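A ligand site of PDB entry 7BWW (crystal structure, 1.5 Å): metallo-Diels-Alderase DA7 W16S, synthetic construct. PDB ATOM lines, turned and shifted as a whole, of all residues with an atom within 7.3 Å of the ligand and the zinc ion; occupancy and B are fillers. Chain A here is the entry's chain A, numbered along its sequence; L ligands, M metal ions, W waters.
Within 4 Å of the zinc ion: Cys 37, His 63 and His 67. The nearest printed residue that does not touch the zinc ion is Met 40 (4.9 Å).
Met 40 touches the ligand (CE to O1, 3.4 Å). Gly 66 touches the ligand. Val 78 touches the ligand (O to C5, 3.6 Å). Gln 82 touches the ligand. Leu 85 touches the ligand. Hydrophobic or aromatic side chains that line the ligand: Met 40, His 63, His 67, Val 78 and Leu 85. Within 4 Å of the ligand: Cys 37, Met 40, His 63, Gly 66, His 67, Val 78, Gln 82 and Leu 85. The nearest printed residue that does not touch the ligand is Ile 81 (4.1 Å).
The zinc ion is bound by an oxygen (O2) of the ligand (2.0 Å), a ring nitrogen (NE2) of His 67 (2.1 Å), a ring nitrogen (NE2) of His 63 (2.1 Å) and the side-chain sulfur of Cys 37 (2.3 Å). The zinc ion has four donor atoms within binding distance.
Water W1 lies within hydrogen-bond range of the side-chain hydroxyl (OH) of Tyr 86 (2.7 Å), an oxygen (O1) of the ligand (2.7 Å) and the backbone carbonyl oxygen (O) of Gln 33 (2.9 Å).
The side-chain amide oxygen of Gln 82 lies within hydrogen-bond range of the side-chain amide nitrogen of Gln 33 (3.2 Å).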
ATOM      1  N   GLN A  33       2.811  -7.855  30.161  1.00  0.00           N
ATOM      2  CA  GLN A  33       2.487  -7.131  28.934  1.00  0.00           C
ATOM      3  C   GLN A  33       3.585  -6.135  28.571  1.00  0.00           C
ATOM      4  O   GLN A  33       3.849  -5.927  27.381  1.00  0.00           O
ATOM      5  CB  GLN A  33       1.137  -6.428  29.088  1.00  0.00           C
ATOM      6  CG  GLN A  33      -0.031  -7.401  29.180  1.00  0.00           C
ATOM      7  CD  GLN A  33      -1.355  -6.709  29.430  1.00  0.00           C
ATOM      8  OE1 GLN A  33      -1.453  -5.785  30.238  1.00  0.00           O
ATOM      9  NE2 GLN A  33      -2.397  -7.169  28.749  1.00  0.00           N
ATOM     10  N   LEU A  34       4.249  -5.532  29.568  1.00  0.00           N
ATOM     11  CA  LEU A  34       5.386  -4.682  29.285  1.00  0.00           C
ATOM     12  C   LEU A  34       6.509  -5.492  28.667  1.00  0.00           C
ATOM     13  O   LEU A  34       7.141  -5.066  27.711  1.00  0.00           O
ATOM     14  CB  LEU A  34       5.864  -3.992  30.568  1.00  0.00           C
ATOM     15  CG  LEU A  34       4.922  -2.971  31.193  1.00  0.00           C
ATOM     16  CD1 LEU A  34       5.389  -2.622  32.603  1.00  0.00           C
ATOM     17  CD2 LEU A  34       4.846  -1.728  30.304  1.00  0.00           C
ATOM     18  N   LEU A  36       6.205  -8.357  26.968  1.00  0.00           N
ATOM     19  CA  LEU A  36       5.808  -8.763  25.617  1.00  0.00           C
ATOM     20  C   LEU A  36       5.992  -7.616  24.619  1.00  0.00           C
ATOM     21  O   LEU A  36       6.430  -7.839  23.484  1.00  0.00           O
ATOM     22  CB  LEU A  36       4.347  -9.226  25.604  1.00  0.00           C
ATOM     23  CG  LEU A  36       3.899  -9.895  24.310  1.00  0.00           C
ATOM     24  CD1 LEU A  36       4.576 -11.246  24.167  1.00  0.00           C
ATOM     25  CD2 LEU A  36       2.366 -10.012  24.271  1.00  0.00           C
ATOM     26  N   CYS A  37       5.621  -6.398  25.026  1.00  0.00           N
ATOM     27  CA  CYS A  37       5.813  -5.238  24.172  1.00  0.00           C
ATOM     28  C   CYS A  37       7.253  -5.151  23.676  1.00  0.00           C
ATOM     29  O   CYS A  37       7.501  -5.081  22.467  1.00  0.00           O
ATOM     30  CB  CYS A  37       5.410  -3.983  24.943  1.00  0.00           C
ATOM     31  SG  CYS A  37       5.974  -2.434  24.178  1.00  0.00           S
ATOM     32  N   GLN A  38       8.208  -5.160  24.612  1.00  0.00           N
ATOM     33  CA  GLN A  38       9.622  -5.058  24.250  1.00  0.00           C
ATOM     34  C   GLN A  38      10.055  -6.206  23.358  1.00  0.00           C
ATOM     35  O   GLN A  38      10.768  -5.998  22.368  1.00  0.00           O
ATOM     36  CB  GLN A  38      10.492  -5.004  25.515  1.00  0.00           C
ATOM     37  CG  GLN A  38      12.009  -4.962  25.260  1.00  0.00           C
ATOM     38  CD  GLN A  38      12.812  -5.758  26.275  1.00  0.00           C
ATOM     39  OE1 GLN A  38      12.311  -6.684  26.919  1.00  0.00           O
ATOM     40  NE2 GLN A  38      14.089  -5.399  26.439  1.00  0.00           N
ATOM     41  N   MET A  40       8.240  -7.920  21.311  1.00  0.00           N
ATOM     42  CA  MET A  40       7.687  -7.734  19.964  1.00  0.00           C
ATOM     43  C   MET A  40       8.494  -6.715  19.161  1.00  0.00           C
ATOM     44  O   MET A  40       8.707  -6.902  17.954  1.00  0.00           O
ATOM     45  CB  MET A  40       6.226  -7.287  20.052  1.00  0.00           C
ATOM     46  CG  MET A  40       5.268  -8.386  20.491  1.00  0.00           C
ATOM     47  SD  MET A  40       3.506  -7.975  20.383  1.00  0.00           S
ATOM     48  CE  MET A  40       3.299  -6.737  21.715  1.00  0.00           C
ATOM     49  N   VAL A  41       8.878  -5.602  19.782  1.00  0.00           N
ATOM     50  CA  VAL A  41       9.725  -4.626  19.099  1.00  0.00           C
ATOM     51  C   VAL A  41      11.002  -5.306  18.599  1.00  0.00           C
ATOM     52  O   VAL A  41      11.421  -5.124  17.452  1.00  0.00           O
ATOM     53  CB  VAL A  41      10.051  -3.437  20.022  1.00  0.00           C
ATOM     54  CG1 VAL A  41      11.055  -2.491  19.352  1.00  0.00           C
ATOM     55  CG2 VAL A  41       8.759  -2.712  20.417  1.00  0.00           C
ATOM     56  N   ILE A  62      -0.313  -3.184  13.800  1.00  0.00           N
ATOM     57  CA  ILE A  62      -1.257  -3.113  14.903  1.00  0.00           C
ATOM     58  C   ILE A  62      -0.529  -2.727  16.187  1.00  0.00           C
ATOM     59  O   ILE A  62      -1.024  -1.911  16.970  1.00  0.00           O
ATOM     60  CB  ILE A  62      -1.993  -4.450  15.044  1.00  0.00           C
ATOM     61  CG1 ILE A  62      -2.917  -4.636  13.832  1.00  0.00           C
ATOM     62  CG2 ILE A  62      -2.793  -4.494  16.328  1.00  0.00           C
ATOM     63  CD1 ILE A  62      -3.375  -6.099  13.674  1.00  0.00           C
ATOM     64  N   HIS A  63       0.666  -3.262  16.396  1.00  0.00           N
ATOM     65  CA  HIS A  63       1.442  -2.849  17.563  1.00  0.00           C
ATOM     66  C   HIS A  63       1.708  -1.340  17.543  1.00  0.00           C
ATOM     67  O   HIS A  63       1.555  -0.664  18.570  1.00  0.00           O
ATOM     68  CB  HIS A  63       2.756  -3.630  17.576  1.00  0.00           C
ATOM     69  CG  HIS A  63       3.531  -3.508  18.849  1.00  0.00           C
ATOM     70  ND1 HIS A  63       4.810  -4.004  18.982  1.00  0.00           N
ATOM     71  CD2 HIS A  63       3.207  -2.980  20.055  1.00  0.00           C
ATOM     72  CE1 HIS A  63       5.254  -3.758  20.198  1.00  0.00           C
ATOM     73  NE2 HIS A  63       4.306  -3.149  20.878  1.00  0.00           N
ATOM     74  N   SER A  64       2.062  -0.798  16.389  1.00  0.00           N
ATOM     75  CA  SER A  64       2.302   0.637  16.258  1.00  0.00           C
ATOM     76  C   SER A  64       1.059   1.449  16.587  1.00  0.00           C
ATOM     77  O   SER A  64       1.116   2.426  17.350  1.00  0.00           O
ATOM     78  CB  SER A  64       2.793   0.951  14.849  1.00  0.00           C
ATOM     79  OG  SER A  64       2.859   2.358  14.648  1.00  0.00           O
ATOM     80  N   PHE A  65      -0.085   1.066  16.024  1.00  0.00           N
ATOM     81  CA  PHE A  65      -1.309   1.788  16.351  1.00  0.00           C
ATOM     82  C   PHE A  65      -1.704   1.617  17.810  1.00  0.00           C
ATOM     83  O   PHE A  65      -2.317   2.521  18.396  1.00  0.00           O
ATOM     84  CB  PHE A  65      -2.436   1.358  15.411  1.00  0.00           C
ATOM     85  CG  PHE A  65      -2.193   1.742  14.001  1.00  0.00           C
ATOM     86  CD1 PHE A  65      -2.007   3.066  13.658  1.00  0.00           C
ATOM     87  CD2 PHE A  65      -2.083   0.781  13.001  1.00  0.00           C
ATOM     88  CE1 PHE A  65      -1.749   3.448  12.341  1.00  0.00           C
ATOM     89  CE2 PHE A  65      -1.817   1.141  11.692  1.00  0.00           C
ATOM     90  CZ  PHE A  65      -1.653   2.476  11.365  1.00  0.00           C
ATOM     91  N   GLY A  66      -1.334   0.489  18.420  1.00  0.00           N
ATOM     92  CA  GLY A  66      -1.547   0.337  19.839  1.00  0.00           C
ATOM     93  C   GLY A  66      -0.779   1.358  20.655  1.00  0.00           C
ATOM     94  O   GLY A  66      -1.290   1.904  21.637  1.00  0.00           O
ATOM     95  N   HIS A  67       0.479   1.618  20.284  1.00  0.00           N
ATOM     96  CA  HIS A  67       1.235   2.661  20.980  1.00  0.00           C
ATOM     97  C   HIS A  67       0.550   4.017  20.839  1.00  0.00           C
ATOM     98  O   HIS A  67       0.475   4.785  21.802  1.00  0.00           O
ATOM     99  CB  HIS A  67       2.667   2.733  20.466  1.00  0.00           C
ATOM    100  CG  HIS A  67       3.566   1.709  21.080  1.00  0.00           C
ATOM    101  ND1 HIS A  67       4.813   2.008  21.584  1.00  0.00           N
ATOM    102  CD2 HIS A  67       3.380   0.380  21.282  1.00  0.00           C
ATOM    103  CE1 HIS A  67       5.355   0.902  22.084  1.00  0.00           C
ATOM    104  NE2 HIS A  67       4.495  -0.091  21.917  1.00  0.00           N
ATOM    105  N   GLN A  68       0.066   4.338  19.637  1.00  0.00           N
ATOM    106  CA  GLN A  68      -0.568   5.626  19.431  1.00  0.00           C
ATOM    107  C   GLN A  68      -1.842   5.756  20.271  1.00  0.00           C
ATOM    108  O   GLN A  68      -2.085   6.812  20.886  1.00  0.00           O
ATOM    109  CB  GLN A  68      -0.858   5.814  17.947  1.00  0.00           C
ATOM    110  CG  GLN A  68       0.410   5.863  17.122  1.00  0.00           C
ATOM    111  CD  GLN A  68       0.146   5.684  15.633  1.00  0.00           C
ATOM    112  OE1 GLN A  68      -0.735   6.315  15.076  1.00  0.00           O
ATOM    113  NE2 GLN A  68       0.892   4.785  15.006  1.00  0.00           N
ATOM    114  N   ALA A  69      -2.623   4.676  20.357  1.00  0.00           N
ATOM    115  CA  ALA A  69      -3.831   4.724  21.180  1.00  0.00           C
ATOM    116  C   ALA A  69      -3.481   4.856  22.653  1.00  0.00           C
ATOM    117  O   ALA A  69      -4.125   5.622  23.379  1.00  0.00           O
ATOM    118  CB  ALA A  69      -4.662   3.445  20.957  1.00  0.00           C
ATOM    119  N   TRP A  70      -2.483   4.116  23.116  1.00  0.00           N
ATOM    120  CA  TRP A  70      -2.080   4.168  24.516  1.00  0.00           C
ATOM    121  C   TRP A  70      -1.605   5.562  24.888  1.00  0.00           C
ATOM    122  O   TRP A  70      -1.940   6.076  25.964  1.00  0.00           O
ATOM    123  CB  TRP A  70      -1.000   3.122  24.774  1.00  0.00           C
ATOM    124  CG  TRP A  70      -0.933   2.609  26.145  1.00  0.00           C
ATOM    125  CD1 TRP A  70      -1.465   1.451  26.617  1.00  0.00           C
ATOM    126  CD2 TRP A  70      -0.240   3.220  27.248  1.00  0.00           C
ATOM    127  NE1 TRP A  70      -1.171   1.308  27.950  1.00  0.00           N
ATOM    128  CE2 TRP A  70      -0.421   2.381  28.366  1.00  0.00           C
ATOM    129  CE3 TRP A  70       0.498   4.400  27.396  1.00  0.00           C
ATOM    130  CZ2 TRP A  70       0.106   2.682  29.619  1.00  0.00           C
ATOM    131  CZ3 TRP A  70       1.020   4.693  28.647  1.00  0.00           C
ATOM    132  CH2 TRP A  70       0.827   3.844  29.738  1.00  0.00           C
ATOM    133  N   GLU A  77      -9.899   1.896  22.619  1.00  0.00           N
ATOM    134  CA  GLU A  77      -9.249   1.394  21.416  1.00  0.00           C
ATOM    135  C   GLU A  77      -8.058   0.532  21.769  1.00  0.00           C
ATOM    136  O   GLU A  77      -7.802  -0.478  21.104  1.00  0.00           O
ATOM    137  CB  GLU A  77      -8.879   2.578  20.513  1.00  0.00           C
ATOM    138  CG  GLU A  77     -10.095   3.432  20.203  1.00  0.00           C
ATOM    139  CD  GLU A  77      -9.981   4.343  18.984  1.00  0.00           C
ATOM    140  OE1 GLU A  77     -10.813   5.257  18.875  1.00  0.00           O
ATOM    141  OE2 GLU A  77      -9.098   4.162  18.125  1.00  0.00           O
ATOM    142  N   VAL A  78      -7.341   0.849  22.851  1.00  0.00           N
ATOM    143  CA  VAL A  78      -6.264  -0.018  23.326  1.00  0.00           C
ATOM    144  C   VAL A  78      -6.761  -1.441  23.537  1.00  0.00           C
ATOM    145  O   VAL A  78      -6.097  -2.408  23.153  1.00  0.00           O
ATOM    146  CB  VAL A  78      -5.640   0.547  24.618  1.00  0.00           C
ATOM    147  CG1 VAL A  78      -4.781  -0.520  25.298  1.00  0.00           C
ATOM    148  CG2 VAL A  78      -4.859   1.802  24.305  1.00  0.00           C
ATOM    149  N   LEU A  79      -7.934  -1.587  24.159  1.00  0.00           N
ATOM    150  CA  LEU A  79      -8.370  -2.920  24.553  1.00  0.00           C
ATOM    151  C   LEU A  79      -8.734  -3.781  23.339  1.00  0.00           C
ATOM    152  O   LEU A  79      -8.452  -4.987  23.345  1.00  0.00           O
ATOM    153  CB  LEU A  79      -9.553  -2.829  25.506  1.00  0.00           C
ATOM    154  CG  LEU A  79      -9.165  -2.221  26.851  1.00  0.00           C
ATOM    155  CD1 LEU A  79     -10.405  -1.966  27.669  1.00  0.00           C
ATOM    156  CD2 LEU A  79      -8.201  -3.136  27.621  1.00  0.00           C
ATOM    157  N   THR A  80      -9.382  -3.204  22.320  1.00  0.00           N
ATOM    158  CA  THR A  80      -9.711  -4.049  21.177  1.00  0.00           C
ATOM    159  C   THR A  80      -8.527  -4.193  20.227  1.00  0.00           C
ATOM    160  O   THR A  80      -8.410  -5.227  19.555  1.00  0.00           O
ATOM    161  CB  THR A  80     -10.950  -3.537  20.457  1.00  0.00           C
ATOM    162  OG1 THR A  80     -10.764  -2.193  20.012  1.00  0.00           O
ATOM    163  CG2 THR A  80     -12.191  -3.626  21.383  1.00  0.00           C
ATOM    164  N   ILE A  81      -7.602  -3.216  20.204  1.00  0.00           N
ATOM    165  CA  ILE A  81      -6.339  -3.440  19.522  1.00  0.00           C
ATOM    166  C   ILE A  81      -5.599  -4.603  20.179  1.00  0.00           C
ATOM    167  O   ILE A  81      -5.056  -5.484  19.485  1.00  0.00           O
ATOM    168  CB  ILE A  81      -5.488  -2.160  19.535  1.00  0.00           C
ATOM    169  CG1 ILE A  81      -6.026  -1.164  18.522  1.00  0.00           C
ATOM    170  CG2 ILE A  81      -4.014  -2.486  19.202  1.00  0.00           C
ATOM    171  CD1 ILE A  81      -5.428   0.275  18.668  1.00  0.00           C
ATOM    172  N   GLN A  82      -5.570  -4.639  21.518  1.00  0.00           N
ATOM    173  CA  GLN A  82      -4.908  -5.735  22.225  1.00  0.00           C
ATOM    174  C   GLN A  82      -5.519  -7.080  21.854  1.00  0.00           C
ATOM    175  O   GLN A  82      -4.788  -8.046  21.594  1.00  0.00           O
ATOM    176  CB  GLN A  82      -4.995  -5.506  23.732  1.00  0.00           C
ATOM    177  CG  GLN A  82      -4.283  -6.599  24.559  1.00  0.00           C
ATOM    178  CD  GLN A  82      -4.722  -6.620  26.019  1.00  0.00           C
ATOM    179  OE1 GLN A  82      -4.780  -7.678  26.641  1.00  0.00           O
ATOM    180  NE2 GLN A  82      -5.045  -5.466  26.552  1.00  0.00           N
ATOM    181  N   GLU A  83      -6.854  -7.161  21.804  1.00  0.00           N
ATOM    182  CA  GLU A  83      -7.497  -8.419  21.440  1.00  0.00           C
ATOM    183  C   GLU A  83      -7.026  -8.878  20.076  1.00  0.00           C
ATOM    184  O   GLU A  83      -6.678 -10.056  19.882  1.00  0.00           O
ATOM    185  CB  GLU A  83      -9.022  -8.275  21.451  1.00  0.00           C
ATOM    186  CG  GLU A  83      -9.626  -8.110  22.835  1.00  0.00           C
ATOM    187  CD  GLU A  83     -11.087  -7.662  22.798  1.00  0.00           C
ATOM    188  OE1 GLU A  83     -11.689  -7.673  21.699  1.00  0.00           O
ATOM    189  OE2 GLU A  83     -11.622  -7.293  23.867  1.00  0.00           O
ATOM    190  N   LEU A  85      -4.236  -7.859  18.338  1.00  0.00           N
ATOM    191  CA  LEU A  85      -2.793  -8.100  18.338  1.00  0.00           C
ATOM    192  C   LEU A  85      -2.453  -9.425  18.986  1.00  0.00           C
ATOM    193  O   LEU A  85      -1.632 -10.194  18.460  1.00  0.00           O
ATOM    194  CB  LEU A  85      -2.101  -6.951  19.092  1.00  0.00           C
ATOM    195  CG  LEU A  85      -0.579  -7.049  19.225  1.00  0.00           C
ATOM    196  CD1 LEU A  85       0.137  -7.078  17.879  1.00  0.00           C
ATOM    197  CD2 LEU A  85      -0.083  -5.868  20.057  1.00  0.00           C
ATOM    198  N   TYR A  86      -3.056  -9.716  20.142  1.00  0.00           N
ATOM    199  CA  TYR A  86      -2.678 -10.922  20.850  1.00  0.00           C
ATOM    200  C   TYR A  86      -3.184 -12.166  20.120  1.00  0.00           C
ATOM    201  O   TYR A  86      -2.498 -13.184  20.123  1.00  0.00           O
ATOM    202  CB  TYR A  86      -3.173 -10.887  22.306  1.00  0.00           C
ATOM    203  CG  TYR A  86      -2.390  -9.946  23.216  1.00  0.00           C
ATOM    204  CD1 TYR A  86      -1.412  -9.076  22.724  1.00  0.00           C
ATOM    205  CD2 TYR A  86      -2.633  -9.931  24.589  1.00  0.00           C
ATOM    206  CE1 TYR A  86      -0.707  -8.207  23.595  1.00  0.00           C
ATOM    207  CE2 TYR A  86      -1.932  -9.105  25.448  1.00  0.00           C
ATOM    208  CZ  TYR A  86      -0.972  -8.235  24.951  1.00  0.00           C
ATOM    209  OH  TYR A  86      -0.294  -7.404  25.848  1.00  0.00           O
HETATM  210  C1  LIG L   1       1.775  -2.937  23.278  1.00  0.00           C
HETATM  211  O1  LIG L   1       2.344  -4.004  23.590  1.00  0.00           O
HETATM  212  O2  LIG L   1       2.453  -1.918  23.060  1.00  0.00           O
HETATM  213  C2  LIG L   1       0.292  -2.840  23.179  1.00  0.00           C
HETATM  214  C3  LIG L   1      -0.476  -3.993  23.261  1.00  0.00           C
HETATM  215  C4  LIG L   1      -1.865  -3.904  23.167  1.00  0.00           C
HETATM  216  C5  LIG L   1      -2.473  -2.663  23.009  1.00  0.00           C
HETATM  217  C6  LIG L   1      -1.708  -1.516  22.910  1.00  0.00           C
HETATM  218  C7  LIG L   1      -0.317  -1.599  23.020  1.00  0.00           C
HETATM  219 ZN    ZN M   1       4.392  -2.032  22.626  1.00  0.00          ZN
HETATM  220  O   HOH W   1       1.942  -6.119  25.223  1.00  0.00           O
